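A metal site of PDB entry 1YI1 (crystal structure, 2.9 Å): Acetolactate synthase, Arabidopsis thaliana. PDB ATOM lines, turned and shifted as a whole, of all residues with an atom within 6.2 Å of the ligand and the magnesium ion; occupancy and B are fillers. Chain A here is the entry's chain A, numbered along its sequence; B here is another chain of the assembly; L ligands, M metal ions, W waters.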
ATOM      1  N   GLY A 399     -25.273   5.372 -23.796  1.00  0.00           N
ATOM      2  CA  GLY A 399     -24.849   6.758 -23.734  1.00  0.00           C
ATOM      3  C   GLY A 399     -23.939   6.983 -24.934  1.00  0.00           C
ATOM      4  O   GLY A 399     -24.062   6.302 -25.944  1.00  0.00           O
ATOM      5  N   VAL A 400     -23.022   7.940 -24.862  1.00  0.00           N
ATOM      6  CA  VAL A 400     -22.120   8.149 -25.998  1.00  0.00           C
ATOM      7  C   VAL A 400     -20.680   8.147 -25.529  1.00  0.00           C
ATOM      8  O   VAL A 400     -20.332   8.800 -24.546  1.00  0.00           O
ATOM      9  CB  VAL A 400     -22.396   9.476 -26.737  1.00  0.00           C
ATOM     10  CG1 VAL A 400     -21.328   9.711 -27.758  1.00  0.00           C
ATOM     11  CG2 VAL A 400     -23.755   9.424 -27.419  1.00  0.00           C
ATOM     12  N   GLY A 401     -19.847   7.392 -26.241  1.00  0.00           N
ATOM     13  CA  GLY A 401     -18.444   7.323 -25.879  1.00  0.00           C
ATOM     14  C   GLY A 401     -17.907   5.904 -25.971  1.00  0.00           C
ATOM     15  O   GLY A 401     -18.406   5.080 -26.738  1.00  0.00           O
ATOM     16  N   GLN A 402     -16.875   5.626 -25.171  1.00  0.00           N
ATOM     17  CA  GLN A 402     -16.264   4.315 -25.188  1.00  0.00           C
ATOM     18  C   GLN A 402     -17.257   3.227 -24.832  1.00  0.00           C
ATOM     19  O   GLN A 402     -17.339   2.212 -25.521  1.00  0.00           O
ATOM     20  CB  GLN A 402     -15.113   4.256 -24.196  1.00  0.00           C
ATOM     21  CG  GLN A 402     -13.967   5.177 -24.478  1.00  0.00           C
ATOM     22  CD  GLN A 402     -12.820   4.938 -23.526  1.00  0.00           C
ATOM     23  OE1 GLN A 402     -12.956   5.090 -22.310  1.00  0.00           O
ATOM     24  NE2 GLN A 402     -11.670   4.540 -24.063  1.00  0.00           N
ATOM     25  N   HIS A 403     -17.998   3.427 -23.746  1.00  0.00           N
ATOM     26  CA  HIS A 403     -18.958   2.414 -23.320  1.00  0.00           C
ATOM     27  C   HIS A 403     -19.922   2.082 -24.451  1.00  0.00           C
ATOM     28  O   HIS A 403     -20.298   0.922 -24.630  1.00  0.00           O
ATOM     29  CB  HIS A 403     -19.722   2.871 -22.070  1.00  0.00           C
ATOM     30  CG  HIS A 403     -20.670   4.018 -22.300  1.00  0.00           C
ATOM     31  ND1 HIS A 403     -22.034   3.893 -22.131  1.00  0.00           N
ATOM     32  CD2 HIS A 403     -20.453   5.316 -22.592  1.00  0.00           C
ATOM     33  CE1 HIS A 403     -22.618   5.065 -22.310  1.00  0.00           C
ATOM     34  NE2 HIS A 403     -21.675   5.948 -22.587  1.00  0.00           N
ATOM     35  N   GLN A 404     -20.288   3.110 -25.213  1.00  0.00           N
ATOM     36  CA  GLN A 404     -21.197   2.933 -26.338  1.00  0.00           C
ATOM     37  C   GLN A 404     -20.574   2.001 -27.377  1.00  0.00           C
ATOM     38  O   GLN A 404     -21.229   1.117 -27.893  1.00  0.00           O
ATOM     39  CB  GLN A 404     -21.508   4.300 -26.960  1.00  0.00           C
ATOM     40  CG  GLN A 404     -22.255   4.258 -28.278  1.00  0.00           C
ATOM     41  CD  GLN A 404     -22.517   5.651 -28.817  1.00  0.00           C
ATOM     42  OE1 GLN A 404     -21.668   6.537 -28.698  1.00  0.00           O
ATOM     43  NE2 GLN A 404     -23.679   5.847 -29.421  1.00  0.00           N
ATOM     44  N   TRP A 406     -18.165  -0.206 -26.800  1.00  0.00           N
ATOM     45  CA  TRP A 406     -18.025  -1.547 -26.284  1.00  0.00           C
ATOM     46  C   TRP A 406     -19.395  -2.222 -26.200  1.00  0.00           C
ATOM     47  O   TRP A 406     -19.510  -3.418 -26.437  1.00  0.00           O
ATOM     48  CB  TRP A 406     -17.325  -1.571 -24.917  1.00  0.00           C
ATOM     49  CG  TRP A 406     -15.868  -1.172 -24.999  1.00  0.00           C
ATOM     50  CD1 TRP A 406     -14.956  -1.553 -25.961  1.00  0.00           C
ATOM     51  CD2 TRP A 406     -15.186  -0.275 -24.128  1.00  0.00           C
ATOM     52  NE1 TRP A 406     -13.750  -0.942 -25.732  1.00  0.00           N
ATOM     53  CE2 TRP A 406     -13.855  -0.147 -24.618  1.00  0.00           C
ATOM     54  CE3 TRP A 406     -15.551   0.441 -22.985  1.00  0.00           C
ATOM     55  CZ2 TRP A 406     -12.909   0.671 -23.993  1.00  0.00           C
ATOM     56  CZ3 TRP A 406     -14.623   1.246 -22.367  1.00  0.00           C
ATOM     57  CH2 TRP A 406     -13.308   1.365 -22.870  1.00  0.00           C
ATOM     58  N   MET A 428     -25.042  12.862 -25.558  1.00  0.00           N
ATOM     59  CA  MET A 428     -24.817  12.272 -24.251  1.00  0.00           C
ATOM     60  C   MET A 428     -26.101  12.401 -23.444  1.00  0.00           C
ATOM     61  O   MET A 428     -26.926  13.267 -23.725  1.00  0.00           O
ATOM     62  CB  MET A 428     -23.686  12.987 -23.504  1.00  0.00           C
ATOM     63  CG  MET A 428     -22.304  12.822 -24.102  1.00  0.00           C
ATOM     64  SD  MET A 428     -21.060  12.856 -22.797  1.00  0.00           S
ATOM     65  CE  MET A 428     -21.487  14.373 -21.927  1.00  0.00           C
ATOM     66  N   ASP A 451     -24.596   2.594 -19.479  1.00  0.00           N
ATOM     67  CA  ASP A 451     -24.168   3.986 -19.425  1.00  0.00           C
ATOM     68  C   ASP A 451     -22.750   4.239 -18.953  1.00  0.00           C
ATOM     69  O   ASP A 451     -22.063   3.339 -18.458  1.00  0.00           O
ATOM     70  CB  ASP A 451     -25.112   4.767 -18.507  1.00  0.00           C
ATOM     71  CG  ASP A 451     -25.905   5.813 -19.240  1.00  0.00           C
ATOM     72  OD1 ASP A 451     -25.306   6.598 -19.999  1.00  0.00           O
ATOM     73  OD2 ASP A 451     -27.135   5.853 -19.045  1.00  0.00           O
ATOM     74  N   GLY A 452     -22.327   5.496 -19.119  1.00  0.00           N
ATOM     75  CA  GLY A 452     -21.019   5.947 -18.691  1.00  0.00           C
ATOM     76  C   GLY A 452     -21.321   6.965 -17.604  1.00  0.00           C
ATOM     77  O   GLY A 452     -22.395   7.560 -17.607  1.00  0.00           O
ATOM     78  N   ASP A 453     -20.392   7.169 -16.677  1.00  0.00           N
ATOM     79  CA  ASP A 453     -20.633   8.103 -15.581  1.00  0.00           C
ATOM     80  C   ASP A 453     -20.858   9.517 -16.058  1.00  0.00           C
ATOM     81  O   ASP A 453     -21.572  10.292 -15.405  1.00  0.00           O
ATOM     82  CB  ASP A 453     -19.507   8.043 -14.536  1.00  0.00           C
ATOM     83  CG  ASP A 453     -18.124   8.247 -15.131  1.00  0.00           C
ATOM     84  OD1 ASP A 453     -17.766   7.509 -16.079  1.00  0.00           O
ATOM     85  OD2 ASP A 453     -17.401   9.141 -14.641  1.00  0.00           O
ATOM     86  N   GLY A 454     -20.273   9.870 -17.205  1.00  0.00           N
ATOM     87  CA  GLY A 454     -20.463  11.214 -17.731  1.00  0.00           C
ATOM     88  C   GLY A 454     -21.862  11.421 -18.283  1.00  0.00           C
ATOM     89  O   GLY A 454     -22.547  12.386 -17.916  1.00  0.00           O
ATOM     90  N   SER A 455     -22.275  10.519 -19.159  1.00  0.00           N
ATOM     91  CA  SER A 455     -23.594  10.575 -19.782  1.00  0.00           C
ATOM     92  C   SER A 455     -24.690  10.373 -18.751  1.00  0.00           C
ATOM     93  O   SER A 455     -25.643  11.150 -18.680  1.00  0.00           O
ATOM     94  CB  SER A 455     -23.731   9.475 -20.839  1.00  0.00           C
ATOM     95  OG  SER A 455     -22.781   9.612 -21.870  1.00  0.00           O
ATOM     96  N   PHE A 456     -24.550   9.322 -17.957  1.00  0.00           N
ATOM     97  CA  PHE A 456     -25.541   9.003 -16.959  1.00  0.00           C
ATOM     98  C   PHE A 456     -25.993  10.201 -16.108  1.00  0.00           C
ATOM     99  O   PHE A 456     -27.191  10.401 -15.886  1.00  0.00           O
ATOM    100  CB  PHE A 456     -25.041   7.882 -16.038  1.00  0.00           C
ATOM    101  CG  PHE A 456     -26.057   7.422 -15.036  1.00  0.00           C
ATOM    102  CD1 PHE A 456     -27.196   6.734 -15.447  1.00  0.00           C
ATOM    103  CD2 PHE A 456     -25.895   7.693 -13.678  1.00  0.00           C
ATOM    104  CE1 PHE A 456     -28.166   6.328 -14.515  1.00  0.00           C
ATOM    105  CE2 PHE A 456     -26.862   7.290 -12.730  1.00  0.00           C
ATOM    106  CZ  PHE A 456     -27.995   6.600 -13.153  1.00  0.00           C
ATOM    107  N   LEU A 478     -21.037   1.740 -16.454  1.00  0.00           N
ATOM    108  CA  LEU A 478     -19.608   1.452 -16.559  1.00  0.00           C
ATOM    109  C   LEU A 478     -18.853   2.701 -16.128  1.00  0.00           C
ATOM    110  O   LEU A 478     -18.442   3.512 -16.959  1.00  0.00           O
ATOM    111  CB  LEU A 478     -19.220   1.084 -17.996  1.00  0.00           C
ATOM    112  CG  LEU A 478     -19.950  -0.108 -18.613  1.00  0.00           C
ATOM    113  CD1 LEU A 478     -19.244  -0.509 -19.904  1.00  0.00           C
ATOM    114  CD2 LEU A 478     -19.988  -1.268 -17.639  1.00  0.00           C
ATOM    115  N   ASN A 479     -18.677   2.853 -14.824  1.00  0.00           N
ATOM    116  CA  ASN A 479     -18.016   4.015 -14.249  1.00  0.00           C
ATOM    117  C   ASN A 479     -16.498   3.978 -14.393  1.00  0.00           C
ATOM    118  O   ASN A 479     -15.847   3.054 -13.893  1.00  0.00           O
ATOM    119  CB  ASN A 479     -18.389   4.128 -12.777  1.00  0.00           C
ATOM    120  CG  ASN A 479     -18.143   5.501 -12.213  1.00  0.00           C
ATOM    121  OD1 ASN A 479     -17.212   6.201 -12.629  1.00  0.00           O
ATOM    122  ND2 ASN A 479     -18.984   5.910 -11.263  1.00  0.00           N
ATOM    123  N   ASN A 480     -15.931   4.977 -15.063  1.00  0.00           N
ATOM    124  CA  ASN A 480     -14.484   5.049 -15.243  1.00  0.00           C
ATOM    125  C   ASN A 480     -13.948   6.447 -14.865  1.00  0.00           C
ATOM    126  O   ASN A 480     -12.868   6.851 -15.316  1.00  0.00           O
ATOM    127  CB  ASN A 480     -14.100   4.675 -16.673  1.00  0.00           C
ATOM    128  CG  ASN A 480     -14.441   5.755 -17.692  1.00  0.00           C
ATOM    129  OD1 ASN A 480     -15.397   6.522 -17.524  1.00  0.00           O
ATOM    130  ND2 ASN A 480     -13.670   5.807 -18.767  1.00  0.00           N
ATOM    131  N   GLN A 481     -14.725   7.176 -14.062  1.00  0.00           N
ATOM    132  CA  GLN A 481     -14.348   8.506 -13.585  1.00  0.00           C
ATOM    133  C   GLN A 481     -13.928   9.521 -14.636  1.00  0.00           C
ATOM    134  O   GLN A 481     -13.507  10.623 -14.277  1.00  0.00           O
ATOM    135  CB  GLN A 481     -13.229   8.379 -12.552  1.00  0.00           C
ATOM    136  CG  GLN A 481     -13.583   7.562 -11.338  1.00  0.00           C
ATOM    137  CD  GLN A 481     -14.787   8.112 -10.598  1.00  0.00           C
ATOM    138  OE1 GLN A 481     -15.927   7.845 -10.955  1.00  0.00           O
ATOM    139  NE2 GLN A 481     -14.524   8.908  -9.553  1.00  0.00           N
ATOM    140  N   HIS A 482     -14.032   9.180 -15.909  1.00  0.00           N
ATOM    141  CA  HIS A 482     -13.620  10.100 -16.967  1.00  0.00           C
ATOM    142  C   HIS A 482     -14.634  10.198 -18.102  1.00  0.00           C
ATOM    143  O   HIS A 482     -15.657   9.522 -18.114  1.00  0.00           O
ATOM    144  CB  HIS A 482     -12.297   9.667 -17.563  1.00  0.00           C
ATOM    145  CG  HIS A 482     -11.119   9.816 -16.646  1.00  0.00           C
ATOM    146  ND1 HIS A 482     -10.961   9.041 -15.522  1.00  0.00           N
ATOM    147  CD2 HIS A 482     -10.057  10.644 -16.691  1.00  0.00           C
ATOM    148  CE1 HIS A 482      -9.846   9.386 -14.906  1.00  0.00           C
ATOM    149  NE2 HIS A 482      -9.271  10.360 -15.591  1.00  0.00           N
ATOM    150  N   LEU A 483     -14.322  11.084 -19.048  1.00  0.00           N
ATOM    151  CA  LEU A 483     -15.119  11.254 -20.263  1.00  0.00           C
ATOM    152  C   LEU A 483     -14.293  10.449 -21.256  1.00  0.00           C
ATOM    153  O   LEU A 483     -13.585  10.996 -22.107  1.00  0.00           O
ATOM    154  CB  LEU A 483     -15.186  12.723 -20.676  1.00  0.00           C
ATOM    155  CG  LEU A 483     -16.123  13.590 -19.839  1.00  0.00           C
ATOM    156  CD1 LEU A 483     -15.960  15.056 -20.221  1.00  0.00           C
ATOM    157  CD2 LEU A 483     -17.559  13.144 -20.074  1.00  0.00           C
ATOM    158  N   GLY A 484     -14.386   9.127 -21.107  1.00  0.00           N
ATOM    159  CA  GLY A 484     -13.651   8.177 -21.919  1.00  0.00           C
ATOM    160  C   GLY A 484     -13.238   8.471 -23.352  1.00  0.00           C
ATOM    161  O   GLY A 484     -12.043   8.578 -23.631  1.00  0.00           O
ATOM    162  N   MET A 485     -14.210   8.586 -24.254  1.00  0.00           N
ATOM    163  CA  MET A 485     -13.872   8.823 -25.648  1.00  0.00           C
ATOM    164  C   MET A 485     -12.997  10.040 -25.873  1.00  0.00           C
ATOM    165  O   MET A 485     -12.089  10.012 -26.686  1.00  0.00           O
ATOM    166  CB  MET A 485     -15.135   8.925 -26.503  1.00  0.00           C
ATOM    167  CG  MET A 485     -14.847   8.829 -28.004  1.00  0.00           C
ATOM    168  SD  MET A 485     -13.752   7.447 -28.419  1.00  0.00           S
ATOM    169  CE  MET A 485     -14.858   6.076 -28.246  1.00  0.00           C
ATOM    170  N   VAL A 486     -13.285  11.125 -25.156  1.00  0.00           N
ATOM    171  CA  VAL A 486     -12.462  12.315 -25.321  1.00  0.00           C
ATOM    172  C   VAL A 486     -11.070  12.017 -24.758  1.00  0.00           C
ATOM    173  O   VAL A 486     -10.063  12.413 -25.332  1.00  0.00           O
ATOM    174  CB  VAL A 486     -13.063  13.523 -24.576  1.00  0.00           C
ATOM    175  CG1 VAL A 486     -12.225  14.762 -24.817  1.00  0.00           C
ATOM    176  CG2 VAL A 486     -14.485  13.752 -25.057  1.00  0.00           C
ATOM    177  N   MET A 487     -11.041  11.282 -23.642  1.00  0.00           N
ATOM    178  CA  MET A 487      -9.797  10.908 -22.981  1.00  0.00           C
ATOM    179  C   MET A 487      -8.906  10.080 -23.905  1.00  0.00           C
ATOM    180  O   MET A 487      -7.702  10.305 -23.974  1.00  0.00           O
ATOM    181  CB  MET A 487     -10.113  10.126 -21.708  1.00  0.00           C
ATOM    182  CG  MET A 487      -8.910   9.709 -20.873  1.00  0.00           C
ATOM    183  SD  MET A 487      -8.867   7.919 -20.573  1.00  0.00           S
ATOM    184  CE  MET A 487     -10.311   7.687 -19.535  1.00  0.00           C
ATOM    185  N   LEU A 503     -13.965  13.389 -14.282  1.00  0.00           N
ATOM    186  CA  LEU A 503     -15.244  13.665 -13.620  1.00  0.00           C
ATOM    187  C   LEU A 503     -15.275  13.453 -12.123  1.00  0.00           C
ATOM    188  O   LEU A 503     -16.286  13.748 -11.487  1.00  0.00           O
ATOM    189  CB  LEU A 503     -16.330  12.814 -14.256  1.00  0.00           C
ATOM    190  CG  LEU A 503     -16.532  13.056 -15.753  1.00  0.00           C
ATOM    191  CD1 LEU A 503     -17.469  12.021 -16.331  1.00  0.00           C
ATOM    192  CD2 LEU A 503     -17.067  14.460 -15.937  1.00  0.00           C
ATOM    193  N   TYR B  33     -17.456  22.608 -21.457  1.00  0.00           N
ATOM    194  CA  TYR B  33     -17.580  21.153 -21.381  1.00  0.00           C
ATOM    195  C   TYR B  33     -16.990  20.584 -22.664  1.00  0.00           C
ATOM    196  O   TYR B  33     -17.525  20.767 -23.754  1.00  0.00           O
ATOM    197  CB  TYR B  33     -19.055  20.762 -21.261  1.00  0.00           C
ATOM    198  CG  TYR B  33     -19.266  19.335 -20.848  1.00  0.00           C
ATOM    199  CD1 TYR B  33     -19.466  19.002 -19.510  1.00  0.00           C
ATOM    200  CD2 TYR B  33     -19.269  18.323 -21.788  1.00  0.00           C
ATOM    201  CE1 TYR B  33     -19.685  17.671 -19.123  1.00  0.00           C
ATOM    202  CE2 TYR B  33     -19.492  16.990 -21.418  1.00  0.00           C
ATOM    203  CZ  TYR B  33     -19.699  16.671 -20.087  1.00  0.00           C
ATOM    204  OH  TYR B  33     -19.941  15.360 -19.724  1.00  0.00           O
HETATM  205  C1  LIG L   1     -17.548  11.295 -23.697  1.00  0.00           C
HETATM  206  C2  LIG L   1     -18.346  10.252 -22.920  1.00  0.00           C
HETATM  207  O1  LIG L   1     -18.015  10.078 -21.617  1.00  0.00           O
HETATM  208  P1  LIG L   1     -18.844   8.952 -20.756  1.00  0.00           P
HETATM  209  O2  LIG L   1     -20.300   9.304 -20.711  1.00  0.00           O
HETATM  210  O3  LIG L   1     -18.338   8.924 -19.354  1.00  0.00           O
HETATM  211  O4  LIG L   1     -18.680   7.494 -21.406  1.00  0.00           O
HETATM  212  P2  LIG L   1     -17.188   7.011 -21.756  1.00  0.00           P
HETATM  213  O5  LIG L   1     -16.721   7.594 -23.046  1.00  0.00           O
HETATM  214  O6  LIG L   1     -16.251   7.321 -20.641  1.00  0.00           O
HETATM  215  O7  LIG L   1     -17.247   5.529 -21.907  1.00  0.00           O
HETATM  216 MG    MG M   1     -17.029   7.853 -18.290  1.00  0.00          MG
HETATM  217  O   HOH W   1     -17.714   5.513 -18.604  1.00  0.00           O
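Val 400 touches the ligand (O to C2, 2.9 Å).
CA of Gly 401 touches O5 of the ligand, 3.3 Å away.
Met 428 touches the ligand.
Gly 452 touches the ligand.
Leu 483 touches the ligand.
Within 4 Å of the ligand: Val 400, Gly 401, Gln 402, His 403, Met 428, Gly 452, Asp 453, Gly 454, Ser 455, Asn 480, His 482, Leu 483, Gly 484 and Met 485.
The nearest printed residue that does not touch the ligand is Val 486 (4.2 Å).
O3 of the ligand is bound to the magnesium ion (2.0 Å).
The magnesium ion is bound by O of His 482 (2.2 Å).
The side-chain amide oxygen (OD1) of Asn 480 is bound to the magnesium ion, at 2.2 Å.
The magnesium ion is bound by OD1 of Asp 453 (2.4 Å).
The magnesium ion is bound by water W1 (2.5 Å).
An oxygen (O6) of the ligand binds the magnesium ion (2.5 Å).
The magnesium ion has six donor atoms within binding distance.
Water W1 lies within hydrogen-bond range of the backbone carbonyl oxygen of Leu 478 (2.7 Å) and an oxygen (O7) of the ligand (3.3 Å).
The backbone NH of Gln 481 lies close to the side-chain carboxylate of Asp 453.
The side-chain hydroxyl (OG) of Ser 455 sits at hydrogen-bond distance from the backbone NH (N) of Val 400 (3.4 Å).
The side-chain hydroxyl of Ser 455 is in hydrogen-bond range of the side-chain sulfur of Met 428 (3.8 Å).
The backbone NH (N) of Val 400 is in hydrogen-bond range of a ring nitrogen (NE2) of His 403.
A ring nitrogen (ND1) of His 403 sits close to the backbone NH of Gly 452 (3.4 Å).
The backbone NH (N) of Gly 401 sits at hydrogen-bond distance from the side-chain amide oxygen (OE1) of Gln 404.
Residues that only touch the magnesium ion: Gly 454 (3.97 Å).
Within 4 Å of the magnesium ion: Asp 453, Gly 454, Asn 480 and His 482.
Along chain A the residues within 4 Å of the magnesium ion span positions 453 to 482.
The nearest printed residue that does not touch the magnesium ion is Gly 484 (4.1 Å).
The backbone NH of Gly 484 lies close to an oxygen (O5) of the ligand.
N of Ser 455 is in hydrogen-bond range of O2 of the ligand (2.8 Å).
An oxygen (O2) of the ligand lies within hydrogen-bond range of the side-chain hydroxyl of Ser 455.
The backbone NH of His 403 lies within hydrogen-bond range of an oxygen (O7) of the ligand (2.9 Å).
The backbone NH (N) of Gln 402 sits at hydrogen-bond distance from an oxygen (O5) of the ligand (2.9 Å).
N of Met 485 lies within hydrogen-bond range of O5 of the ligand, 3.0 Å away.
An oxygen (O3) of the ligand lies close to the backbone NH (N) of Gly 454 (3.0 Å).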
